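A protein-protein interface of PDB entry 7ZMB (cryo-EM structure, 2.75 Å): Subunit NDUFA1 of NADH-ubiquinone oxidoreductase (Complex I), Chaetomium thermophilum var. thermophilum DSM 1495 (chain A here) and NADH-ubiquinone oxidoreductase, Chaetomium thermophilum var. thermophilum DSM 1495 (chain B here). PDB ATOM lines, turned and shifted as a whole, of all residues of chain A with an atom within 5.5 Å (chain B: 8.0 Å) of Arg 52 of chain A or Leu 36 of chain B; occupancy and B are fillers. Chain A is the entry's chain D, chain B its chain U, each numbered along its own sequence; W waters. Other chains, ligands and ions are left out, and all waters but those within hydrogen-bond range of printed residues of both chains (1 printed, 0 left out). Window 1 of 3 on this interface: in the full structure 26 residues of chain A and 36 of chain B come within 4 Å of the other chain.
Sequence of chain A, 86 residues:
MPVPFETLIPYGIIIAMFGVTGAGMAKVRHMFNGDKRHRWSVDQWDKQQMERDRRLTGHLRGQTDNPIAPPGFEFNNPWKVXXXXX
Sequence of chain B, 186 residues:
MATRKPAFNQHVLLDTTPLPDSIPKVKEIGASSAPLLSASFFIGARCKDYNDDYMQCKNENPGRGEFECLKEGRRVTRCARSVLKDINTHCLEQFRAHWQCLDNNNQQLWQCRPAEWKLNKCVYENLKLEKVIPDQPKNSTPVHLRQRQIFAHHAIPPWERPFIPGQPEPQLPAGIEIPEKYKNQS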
ATOM      1  N   LYS A  47      23.272 -20.713  -8.135  1.00  0.00           N
ATOM      2  CA  LYS A  47      22.992 -22.081  -7.653  1.00  0.00           C
ATOM      3  C   LYS A  47      21.651 -22.538  -8.226  1.00  0.00           C
ATOM      4  O   LYS A  47      21.596 -23.677  -8.721  1.00  0.00           O
ATOM      5  CB  LYS A  47      22.921 -22.047  -6.129  1.00  0.00           C
ATOM      6  CG  LYS A  47      24.246 -22.114  -5.389  1.00  0.00           C
ATOM      7  CD  LYS A  47      24.070 -21.941  -3.900  1.00  0.00           C
ATOM      8  CE  LYS A  47      25.360 -21.578  -3.196  1.00  0.00           C
ATOM      9  NZ  LYS A  47      25.888 -20.277  -3.667  1.00  0.00           N
ATOM     10  N   GLN A  48      20.636 -21.668  -8.203  1.00  0.00           N
ATOM     11  CA  GLN A  48      19.297 -21.986  -8.769  1.00  0.00           C
ATOM     12  C   GLN A  48      19.381 -22.156 -10.287  1.00  0.00           C
ATOM     13  O   GLN A  48      18.758 -23.086 -10.798  1.00  0.00           O
ATOM     14  CB  GLN A  48      18.305 -20.882  -8.404  1.00  0.00           C
ATOM     15  CG  GLN A  48      17.833 -20.900  -6.965  1.00  0.00           C
ATOM     16  CD  GLN A  48      16.858 -19.773  -6.737  1.00  0.00           C
ATOM     17  OE1 GLN A  48      16.319 -19.202  -7.680  1.00  0.00           O
ATOM     18  NE2 GLN A  48      16.610 -19.458  -5.477  1.00  0.00           N
ATOM     19  N   GLN A  49      20.103 -21.275 -10.978  1.00  0.00           N
ATOM     20  CA  GLN A  49      20.259 -21.347 -12.459  1.00  0.00           C
ATOM     21  C   GLN A  49      20.988 -22.635 -12.866  1.00  0.00           C
ATOM     22  O   GLN A  49      20.632 -23.186 -13.914  1.00  0.00           O
ATOM     23  CB  GLN A  49      20.969 -20.099 -12.992  1.00  0.00           C
ATOM     24  CG  GLN A  49      20.104 -18.848 -13.025  1.00  0.00           C
ATOM     25  CD  GLN A  49      19.200 -18.760 -14.232  1.00  0.00           C
ATOM     26  OE1 GLN A  49      19.094 -19.686 -15.030  1.00  0.00           O
ATOM     27  NE2 GLN A  49      18.537 -17.627 -14.375  1.00  0.00           N
ATOM     28  N   MET A  50      21.971 -23.089 -12.080  1.00  0.00           N
ATOM     29  CA  MET A  50      22.698 -24.363 -12.358  1.00  0.00           C
ATOM     30  C   MET A  50      21.751 -25.551 -12.213  1.00  0.00           C
ATOM     31  O   MET A  50      21.901 -26.526 -12.958  1.00  0.00           O
ATOM     32  CB  MET A  50      23.940 -24.556 -11.479  1.00  0.00           C
ATOM     33  CG  MET A  50      25.156 -23.851 -12.040  1.00  0.00           C
ATOM     34  SD  MET A  50      26.636 -23.971 -11.018  1.00  0.00           S
ATOM     35  CE  MET A  50      26.163 -22.943  -9.631  1.00  0.00           C
ATOM     36  N   GLU A  51      20.799 -25.450 -11.293  1.00  0.00           N
ATOM     37  CA  GLU A  51      19.872 -26.577 -11.064  1.00  0.00           C
ATOM     38  C   GLU A  51      18.849 -26.537 -12.192  1.00  0.00           C
ATOM     39  O   GLU A  51      18.368 -27.609 -12.578  1.00  0.00           O
ATOM     40  CB  GLU A  51      19.177 -26.410  -9.719  1.00  0.00           C
ATOM     41  CG  GLU A  51      20.060 -26.718  -8.530  1.00  0.00           C
ATOM     42  CD  GLU A  51      19.479 -26.201  -7.225  1.00  0.00           C
ATOM     43  OE1 GLU A  51      18.736 -25.203  -7.273  1.00  0.00           O
ATOM     44  OE2 GLU A  51      19.759 -26.806  -6.173  1.00  0.00           O
ATOM     45  N   ARG A  52      18.628 -25.353 -12.761  1.00  0.00           N
ATOM     46  CA  ARG A  52      17.656 -25.233 -13.871  1.00  0.00           C
ATOM     47  C   ARG A  52      18.333 -25.705 -15.164  1.00  0.00           C
ATOM     48  O   ARG A  52      17.616 -25.981 -16.123  1.00  0.00           O
ATOM     49  CB  ARG A  52      17.044 -23.828 -13.925  1.00  0.00           C
ATOM     50  CG  ARG A  52      15.713 -23.785 -14.659  1.00  0.00           C
ATOM     51  CD  ARG A  52      15.119 -22.403 -14.826  1.00  0.00           C
ATOM     52  NE  ARG A  52      14.224 -22.383 -15.973  1.00  0.00           N
ATOM     53  CZ  ARG A  52      14.588 -22.040 -17.201  1.00  0.00           C
ATOM     54  NH1 ARG A  52      15.833 -21.668 -17.444  1.00  0.00           N
ATOM     55  NH2 ARG A  52      13.705 -22.060 -18.182  1.00  0.00           N
ATOM     56  N   ASP A  53      19.652 -25.893 -15.143  1.00  0.00           N
ATOM     57  CA  ASP A  53      20.385 -26.405 -16.332  1.00  0.00           C
ATOM     58  C   ASP A  53      20.317 -27.927 -16.262  1.00  0.00           C
ATOM     59  O   ASP A  53      20.154 -28.553 -17.312  1.00  0.00           O
ATOM     60  CB  ASP A  53      21.822 -25.885 -16.371  1.00  0.00           C
ATOM     61  CG  ASP A  53      21.927 -24.412 -16.719  1.00  0.00           C
ATOM     62  OD1 ASP A  53      20.875 -23.780 -16.911  1.00  0.00           O
ATOM     63  OD2 ASP A  53      23.062 -23.914 -16.793  1.00  0.00           O
ATOM     64  N   ARG A  54      20.427 -28.481 -15.058  1.00  0.00           N
ATOM     65  CA  ARG A  54      20.243 -29.940 -14.854  1.00  0.00           C
ATOM     66  C   ARG A  54      18.826 -30.324 -15.276  1.00  0.00           C
ATOM     67  O   ARG A  54      18.669 -31.391 -15.868  1.00  0.00           O
ATOM     68  CB  ARG A  54      20.523 -30.287 -13.396  1.00  0.00           C
ATOM     69  CG  ARG A  54      20.771 -31.764 -13.138  1.00  0.00           C
ATOM     70  CD  ARG A  54      20.482 -32.111 -11.695  1.00  0.00           C
ATOM     71  NE  ARG A  54      21.627 -32.001 -10.807  1.00  0.00           N
ATOM     72  CZ  ARG A  54      21.536 -31.941  -9.488  1.00  0.00           C
ATOM     73  NH1 ARG A  54      22.627 -31.863  -8.749  1.00  0.00           N
ATOM     74  NH2 ARG A  54      20.348 -31.948  -8.913  1.00  0.00           N
ATOM     75  N   ARG A  55      17.839 -29.476 -14.991  1.00  0.00           N
ATOM     76  CA  ARG A  55      16.437 -29.745 -15.381  1.00  0.00           C
ATOM     77  C   ARG A  55      16.289 -29.849 -16.905  1.00  0.00           C
ATOM     78  O   ARG A  55      15.395 -30.578 -17.346  1.00  0.00           O
ATOM     79  CB  ARG A  55      15.499 -28.708 -14.767  1.00  0.00           C
ATOM     80  CG  ARG A  55      15.340 -28.805 -13.260  1.00  0.00           C
ATOM     81  CD  ARG A  55      14.509 -27.617 -12.836  1.00  0.00           C
ATOM     82  NE  ARG A  55      13.201 -27.669 -13.465  1.00  0.00           N
ATOM     83  CZ  ARG A  55      12.363 -26.648 -13.531  1.00  0.00           C
ATOM     84  NH1 ARG A  55      12.700 -25.481 -13.011  1.00  0.00           N
ATOM     85  NH2 ARG A  55      11.191 -26.796 -14.119  1.00  0.00           N
ATOM     86  N   LEU A  56      17.127 -29.146 -17.669  1.00  0.00           N
ATOM     87  CA  LEU A  56      17.035 -29.167 -19.151  1.00  0.00           C
ATOM     88  C   LEU A  56      18.091 -30.081 -19.787  1.00  0.00           C
ATOM     89  O   LEU A  56      17.871 -30.482 -20.928  1.00  0.00           O
ATOM     90  CB  LEU A  56      17.183 -27.733 -19.661  1.00  0.00           C
ATOM     91  CG  LEU A  56      16.107 -26.737 -19.239  1.00  0.00           C
ATOM     92  CD1 LEU A  56      16.691 -25.351 -19.031  1.00  0.00           C
ATOM     93  CD2 LEU A  56      14.991 -26.689 -20.263  1.00  0.00           C
ATOM     94  N   PHE A  73       9.327 -31.014 -18.315  1.00  0.00           N
ATOM     95  CA  PHE A  73      10.152 -30.000 -17.611  1.00  0.00           C
ATOM     96  C   PHE A  73       9.255 -29.316 -16.581  1.00  0.00           C
ATOM     97  O   PHE A  73       9.756 -28.866 -15.535  1.00  0.00           O
ATOM     98  CB  PHE A  73      10.779 -29.047 -18.626  1.00  0.00           C
ATOM     99  CG  PHE A  73      11.519 -27.872 -18.046  1.00  0.00           C
ATOM    100  CD1 PHE A  73      12.804 -28.015 -17.549  1.00  0.00           C
ATOM    101  CD2 PHE A  73      10.936 -26.615 -18.019  1.00  0.00           C
ATOM    102  CE1 PHE A  73      13.483 -26.929 -17.024  1.00  0.00           C
ATOM    103  CE2 PHE A  73      11.621 -25.531 -17.499  1.00  0.00           C
ATOM    104  CZ  PHE A  73      12.892 -25.689 -17.001  1.00  0.00           C
ATOM    105  N   GLU B  28       6.879 -24.071 -21.669  1.00  0.00           N
ATOM    106  CA  GLU B  28       7.868 -23.285 -20.889  1.00  0.00           C
ATOM    107  C   GLU B  28       9.115 -22.960 -21.721  1.00  0.00           C
ATOM    108  O   GLU B  28       9.397 -23.680 -22.683  1.00  0.00           O
ATOM    109  CB  GLU B  28       8.251 -24.025 -19.613  1.00  0.00           C
ATOM    110  CG  GLU B  28       7.075 -24.438 -18.746  1.00  0.00           C
ATOM    111  CD  GLU B  28       6.399 -23.342 -17.940  1.00  0.00           C
ATOM    112  OE1 GLU B  28       6.882 -22.194 -17.961  1.00  0.00           O
ATOM    113  OE2 GLU B  28       5.385 -23.643 -17.288  1.00  0.00           O
ATOM    114  N   ILE B  29       9.817 -21.886 -21.366  1.00  0.00           N
ATOM    115  CA  ILE B  29      11.090 -21.517 -22.053  1.00  0.00           C
ATOM    116  C   ILE B  29      12.059 -22.673 -21.864  1.00  0.00           C
ATOM    117  O   ILE B  29      12.165 -23.171 -20.735  1.00  0.00           O
ATOM    118  CB  ILE B  29      11.664 -20.225 -21.433  1.00  0.00           C
ATOM    119  CG1 ILE B  29      10.752 -19.018 -21.649  1.00  0.00           C
ATOM    120  CG2 ILE B  29      13.079 -19.964 -21.926  1.00  0.00           C
ATOM    121  CD1 ILE B  29      10.526 -18.693 -23.095  1.00  0.00           C
ATOM    122  N   GLY B  30      12.758 -23.058 -22.926  1.00  0.00           N
ATOM    123  CA  GLY B  30      13.684 -24.199 -22.859  1.00  0.00           C
ATOM    124  C   GLY B  30      15.129 -23.787 -22.806  1.00  0.00           C
ATOM    125  O   GLY B  30      15.979 -24.676 -22.782  1.00  0.00           O
ATOM    126  N   ALA B  31      15.402 -22.489 -22.828  1.00  0.00           N
ATOM    127  CA  ALA B  31      16.768 -21.990 -22.799  1.00  0.00           C
ATOM    128  C   ALA B  31      17.373 -22.136 -21.410  1.00  0.00           C
ATOM    129  O   ALA B  31      16.683 -22.035 -20.393  1.00  0.00           O
ATOM    130  CB  ALA B  31      16.821 -20.530 -23.241  1.00  0.00           C
ATOM    131  N   SER B  32      18.693 -22.358 -21.391  1.00  0.00           N
ATOM    132  CA  SER B  32      19.451 -22.534 -20.125  1.00  0.00           C
ATOM    133  C   SER B  32      20.050 -21.199 -19.667  1.00  0.00           C
ATOM    134  O   SER B  32      19.856 -20.206 -20.382  1.00  0.00           O
ATOM    135  CB  SER B  32      20.504 -23.576 -20.307  1.00  0.00           C
ATOM    136  OG  SER B  32      21.385 -23.189 -21.341  1.00  0.00           O
ATOM    137  N   SER B  33      20.794 -21.187 -18.557  1.00  0.00           N
ATOM    138  CA  SER B  33      21.343 -19.937 -17.955  1.00  0.00           C
ATOM    139  C   SER B  33      22.173 -19.061 -18.903  1.00  0.00           C
ATOM    140  O   SER B  33      21.912 -17.854 -18.924  1.00  0.00           O
ATOM    141  CB  SER B  33      22.115 -20.263 -16.702  1.00  0.00           C
ATOM    142  OG  SER B  33      23.177 -21.163 -16.977  1.00  0.00           O
ATOM    143  N   ALA B  34      23.168 -19.613 -19.609  1.00  0.00           N
ATOM    144  CA  ALA B  34      24.073 -18.779 -20.436  1.00  0.00           C
ATOM    145  C   ALA B  34      23.331 -18.158 -21.617  1.00  0.00           C
ATOM    146  O   ALA B  34      23.454 -16.937 -21.798  1.00  0.00           O
ATOM    147  CB  ALA B  34      25.314 -19.533 -20.834  1.00  0.00           C
ATOM    148  N   PRO B  35      22.495 -18.896 -22.378  1.00  0.00           N
ATOM    149  CA  PRO B  35      21.689 -18.284 -23.425  1.00  0.00           C
ATOM    150  C   PRO B  35      20.751 -17.215 -22.847  1.00  0.00           C
ATOM    151  O   PRO B  35      20.606 -16.205 -23.497  1.00  0.00           O
ATOM    152  CB  PRO B  35      20.939 -19.457 -24.066  1.00  0.00           C
ATOM    153  CG  PRO B  35      21.800 -20.650 -23.774  1.00  0.00           C
ATOM    154  CD  PRO B  35      22.381 -20.360 -22.411  1.00  0.00           C
ATOM    155  N   LEU B  36      20.122 -17.449 -21.687  1.00  0.00           N
ATOM    156  CA  LEU B  36      19.143 -16.447 -21.166  1.00  0.00           C
ATOM    157  C   LEU B  36      19.814 -15.120 -20.775  1.00  0.00           C
ATOM    158  O   LEU B  36      19.187 -14.088 -20.997  1.00  0.00           O
ATOM    159  CB  LEU B  36      18.084 -17.013 -20.203  1.00  0.00           C
ATOM    160  CG  LEU B  36      18.529 -17.783 -18.964  1.00  0.00           C
ATOM    161  CD1 LEU B  36      19.051 -16.854 -17.884  1.00  0.00           C
ATOM    162  CD2 LEU B  36      17.369 -18.601 -18.419  1.00  0.00           C
ATOM    163  N   LEU B  37      21.034 -15.139 -20.233  1.00  0.00           N
ATOM    164  CA  LEU B  37      21.812 -13.906 -19.915  1.00  0.00           C
ATOM    165  C   LEU B  37      22.213 -13.165 -21.194  1.00  0.00           C
ATOM    166  O   LEU B  37      22.216 -11.923 -21.166  1.00  0.00           O
ATOM    167  CB  LEU B  37      23.021 -14.278 -19.053  1.00  0.00           C
ATOM    168  CG  LEU B  37      24.045 -13.181 -18.790  1.00  0.00           C
ATOM    169  CD1 LEU B  37      23.499 -12.176 -17.795  1.00  0.00           C
ATOM    170  CD2 LEU B  37      25.335 -13.786 -18.266  1.00  0.00           C
ATOM    171  N   SER B  38      22.474 -13.879 -22.290  1.00  0.00           N
ATOM    172  CA  SER B  38      22.926 -13.245 -23.557  1.00  0.00           C
ATOM    173  C   SER B  38      21.720 -12.629 -24.274  1.00  0.00           C
ATOM    174  O   SER B  38      21.917 -11.740 -25.112  1.00  0.00           O
ATOM    175  CB  SER B  38      23.652 -14.214 -24.449  1.00  0.00           C
ATOM    176  OG  SER B  38      23.047 -15.488 -24.431  1.00  0.00           O
ATOM    177  N   ALA B  39      20.516 -13.083 -23.933  1.00  0.00           N
ATOM    178  CA  ALA B  39      19.299 -12.571 -24.535  1.00  0.00           C
ATOM    179  C   ALA B  39      18.497 -11.688 -23.594  1.00  0.00           C
ATOM    180  O   ALA B  39      17.430 -11.211 -23.983  1.00  0.00           O
ATOM    181  CB  ALA B  39      18.428 -13.728 -25.028  1.00  0.00           C
ATOM    182  N   SER B  40      18.992 -11.447 -22.378  1.00  0.00           N
ATOM    183  CA  SER B  40      18.204 -10.741 -21.371  1.00  0.00           C
ATOM    184  C   SER B  40      17.923  -9.305 -21.790  1.00  0.00           C
ATOM    185  O   SER B  40      16.783  -8.836 -21.708  1.00  0.00           O
ATOM    186  CB  SER B  40      18.924 -10.776 -20.022  1.00  0.00           C
ATOM    187  OG  SER B  40      20.158 -10.092 -20.083  1.00  0.00           O
ATOM    188  N   PHE B  41      18.950  -8.591 -22.242  1.00  0.00           N
ATOM    189  CA  PHE B  41      18.766  -7.208 -22.657  1.00  0.00           C
ATOM    190  C   PHE B  41      17.941  -7.081 -23.927  1.00  0.00           C
ATOM    191  O   PHE B  41      17.520  -5.970 -24.258  1.00  0.00           O
ATOM    192  CB  PHE B  41      20.123  -6.536 -22.837  1.00  0.00           C
ATOM    193  CG  PHE B  41      20.816  -6.257 -21.550  1.00  0.00           C
ATOM    194  CD1 PHE B  41      20.410  -5.211 -20.751  1.00  0.00           C
ATOM    195  CD2 PHE B  41      21.845  -7.060 -21.120  1.00  0.00           C
ATOM    196  CE1 PHE B  41      21.029  -4.961 -19.566  1.00  0.00           C
ATOM    197  CE2 PHE B  41      22.465  -6.815 -19.932  1.00  0.00           C
ATOM    198  CZ  PHE B  41      22.055  -5.764 -19.154  1.00  0.00           C
ATOM    199  N   PHE B  42      17.710  -8.181 -24.640  1.00  0.00           N
ATOM    200  CA  PHE B  42      16.760  -8.181 -25.738  1.00  0.00           C
ATOM    201  C   PHE B  42      15.376  -8.622 -25.295  1.00  0.00           C
ATOM    202  O   PHE B  42      14.381  -8.150 -25.850  1.00  0.00           O
ATOM    203  CB  PHE B  42      17.278  -9.067 -26.875  1.00  0.00           C
ATOM    204  CG  PHE B  42      18.677  -8.732 -27.297  1.00  0.00           C
ATOM    205  CD1 PHE B  42      19.001  -7.436 -27.678  1.00  0.00           C
ATOM    206  CD2 PHE B  42      19.668  -9.692 -27.291  1.00  0.00           C
ATOM    207  CE1 PHE B  42      20.284  -7.106 -28.051  1.00  0.00           C
ATOM    208  CE2 PHE B  42      20.961  -9.374 -27.670  1.00  0.00           C
ATOM    209  CZ  PHE B  42      21.273  -8.081 -28.045  1.00  0.00           C
ATOM    210  N   ILE B  43      15.284  -9.499 -24.296  1.00  0.00           N
ATOM    211  CA  ILE B  43      13.994  -9.748 -23.663  1.00  0.00           C
ATOM    212  C   ILE B  43      13.460  -8.463 -23.047  1.00  0.00           C
ATOM    213  O   ILE B  43      12.292  -8.104 -23.224  1.00  0.00           O
ATOM    214  CB  ILE B  43      14.109 -10.854 -22.603  1.00  0.00           C
ATOM    215  CG1 ILE B  43      14.403 -12.202 -23.253  1.00  0.00           C
ATOM    216  CG2 ILE B  43      12.842 -10.906 -21.770  1.00  0.00           C
ATOM    217  CD1 ILE B  43      14.978 -13.207 -22.314  1.00  0.00           C
ATOM    218  N   LEU B  84      13.619 -15.307 -28.217  1.00  0.00           N
ATOM    219  CA  LEU B  84      14.507 -16.455 -28.350  1.00  0.00           C
ATOM    220  C   LEU B  84      14.415 -17.055 -29.743  1.00  0.00           C
ATOM    221  O   LEU B  84      15.436 -17.387 -30.357  1.00  0.00           O
ATOM    222  CB  LEU B  84      14.169 -17.509 -27.297  1.00  0.00           C
ATOM    223  CG  LEU B  84      14.497 -17.243 -25.833  1.00  0.00           C
ATOM    224  CD1 LEU B  84      13.588 -18.050 -24.953  1.00  0.00           C
ATOM    225  CD2 LEU B  84      15.935 -17.577 -25.539  1.00  0.00           C
ATOM    226  N   ILE B  87      16.026 -14.429 -32.212  1.00  0.00           N
ATOM    227  CA  ILE B  87      17.480 -14.501 -32.171  1.00  0.00           C
ATOM    228  C   ILE B  87      17.966 -15.760 -32.876  1.00  0.00           C
ATOM    229  O   ILE B  87      19.004 -15.755 -33.544  1.00  0.00           O
ATOM    230  CB  ILE B  87      17.971 -14.439 -30.712  1.00  0.00           C
ATOM    231  CG1 ILE B  87      17.607 -13.100 -30.083  1.00  0.00           C
ATOM    232  CG2 ILE B  87      19.457 -14.671 -30.630  1.00  0.00           C
ATOM    233  CD1 ILE B  87      17.346 -13.177 -28.614  1.00  0.00           C
ATOM    234  N   PHE B  95      24.810 -15.644 -31.525  1.00  0.00           N
ATOM    235  CA  PHE B  95      24.209 -15.909 -30.228  1.00  0.00           C
ATOM    236  C   PHE B  95      24.913 -17.061 -29.534  1.00  0.00           C
ATOM    237  O   PHE B  95      25.256 -16.968 -28.353  1.00  0.00           O
ATOM    238  CB  PHE B  95      22.721 -16.192 -30.407  1.00  0.00           C
ATOM    239  CG  PHE B  95      21.994 -16.444 -29.125  1.00  0.00           C
ATOM    240  CD1 PHE B  95      21.979 -15.491 -28.123  1.00  0.00           C
ATOM    241  CD2 PHE B  95      21.327 -17.628 -28.924  1.00  0.00           C
ATOM    242  CE1 PHE B  95      21.317 -15.721 -26.961  1.00  0.00           C
ATOM    243  CE2 PHE B  95      20.664 -17.859 -27.756  1.00  0.00           C
ATOM    244  CZ  PHE B  95      20.658 -16.907 -26.776  1.00  0.00           C
ATOM    245  N   TRP B  99      27.005 -16.858 -25.780  1.00  0.00           N
ATOM    246  CA  TRP B  99      26.682 -17.552 -24.539  1.00  0.00           C
ATOM    247  C   TRP B  99      27.595 -18.740 -24.283  1.00  0.00           C
ATOM    248  O   TRP B  99      27.645 -19.229 -23.151  1.00  0.00           O
ATOM    249  CB  TRP B  99      25.204 -17.981 -24.489  1.00  0.00           C
ATOM    250  CG  TRP B  99      24.717 -18.996 -25.492  1.00  0.00           C
ATOM    251  CD1 TRP B  99      23.904 -18.759 -26.551  1.00  0.00           C
ATOM    252  CD2 TRP B  99      24.977 -20.404 -25.499  1.00  0.00           C
ATOM    253  NE1 TRP B  99      23.657 -19.920 -27.235  1.00  0.00           N
ATOM    254  CE2 TRP B  99      24.305 -20.945 -26.608  1.00  0.00           C
ATOM    255  CE3 TRP B  99      25.718 -21.257 -24.684  1.00  0.00           C
ATOM    256  CZ2 TRP B  99      24.353 -22.296 -26.918  1.00  0.00           C
ATOM    257  CZ3 TRP B  99      25.765 -22.590 -24.992  1.00  0.00           C
ATOM    258  CH2 TRP B  99      25.090 -23.101 -26.098  1.00  0.00           C
ATOM    259  N   LEU B 102      30.339 -17.036 -22.458  1.00  0.00           N
ATOM    260  CA  LEU B 102      29.792 -16.709 -21.119  1.00  0.00           C
ATOM    261  C   LEU B 102      29.866 -17.941 -20.226  1.00  0.00           C
ATOM    262  O   LEU B 102      30.155 -17.781 -19.040  1.00  0.00           O
ATOM    263  CB  LEU B 102      28.341 -16.257 -21.292  1.00  0.00           C
ATOM    264  CG  LEU B 102      28.142 -14.798 -21.694  1.00  0.00           C
ATOM    265  CD1 LEU B 102      26.678 -14.520 -21.982  1.00  0.00           C
ATOM    266  CD2 LEU B 102      28.659 -13.863 -20.611  1.00  0.00           C
ATOM    267  N   GLN B 107      29.879 -16.616 -16.439  1.00  0.00           N
ATOM    268  CA  GLN B 107      28.678 -15.811 -16.782  1.00  0.00           C
ATOM    269  C   GLN B 107      28.952 -14.327 -16.518  1.00  0.00           C
ATOM    270  O   GLN B 107      28.000 -13.592 -16.226  1.00  0.00           O
ATOM    271  CB  GLN B 107      27.411 -16.444 -16.198  1.00  0.00           C
ATOM    272  CG  GLN B 107      27.112 -17.792 -16.836  1.00  0.00           C
ATOM    273  CD  GLN B 107      25.733 -18.324 -16.537  1.00  0.00           C
ATOM    274  OE1 GLN B 107      24.912 -17.672 -15.897  1.00  0.00           O
ATOM    275  NE2 GLN B 107      25.470 -19.530 -17.008  1.00  0.00           N
HETATM  276  O   HOH W   1      18.720 -22.179 -16.298  1.00  0.00           O
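O of Ile 29 of chain B lies within hydrogen-bond range of NH2 of Arg 52 of chain A, 3.2 Å away. The backbone carbonyl oxygen (O) of Ala 31 of chain B lies within hydrogen-bond range of the guanidinium group (NH1) of Arg 52 of chain A (3.1 Å). The side-chain hydroxyl (OG) of Ser 33 of chain B sits at hydrogen-bond distance from the side-chain carboxylate (OD2) of Asp 53 of chain A, 2.8 Å away.
The side-chain amide nitrogen (NE2) of Gln 107 of chain B is in hydrogen-bond range of the side-chain hydroxyl (OG) of Ser 33 of chain B, 2.8 Å away.
Among the printed residues, merely in contact across the chains: Leu 56 of chain A with Gly 30 of chain B, Asp 53 of chain A with Ser 32 of chain B, Gln 49 of chain A with Ser 33 of chain B, Arg 52 of chain A with Leu 36 of chain B, Leu 56 of chain A with Ala 31 of chain B and Gln 49 of chain A with Leu 36 of chain B.
Arg 52 of chain A touches three residues of chain B. Leu 36 of chain B touches just these residues of chain A: Gln 49 and Arg 52. Of the printed residues of chain A, Gly 30 of chain B touches Leu 56. Of the printed residues of chain A, Ile 29 of chain B touches Arg 52. Printed residues of chain A within 4 Å of Ala 31 of chain B: Arg 52 (3.1 Å) and Leu 56 (3.6 Å). Of the printed residues of chain A, Ser 32 of chain B touches Asp 53. Arg 54 of chain A touches none of the printed residues of chain B. Gln 107 of chain B touches none of the printed residues of chain A. The nearest printed residue of chain A that does not touch Ser 32 of chain B is Leu 56 of chain A (4.1 Å).
Of the 11 printed residues of chain A, 4 touch a printed residue of chain B. Among the printed residues, 9 pairs touch across the chains. Among the printed residues, no Asp or Glu carboxylate lies within 4 Å of a Lys or Arg side-chain nitrogen of the other chain.
Water W1 lies within hydrogen-bond range of OD1 of Asp 53 of chain A (2.8 Å), OE1 of Gln 49 of chain A (2.8 Å), NH1 of Arg 52 of chain A (3.1 Å) and N of Ser 33 of chain B (3.2 Å).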
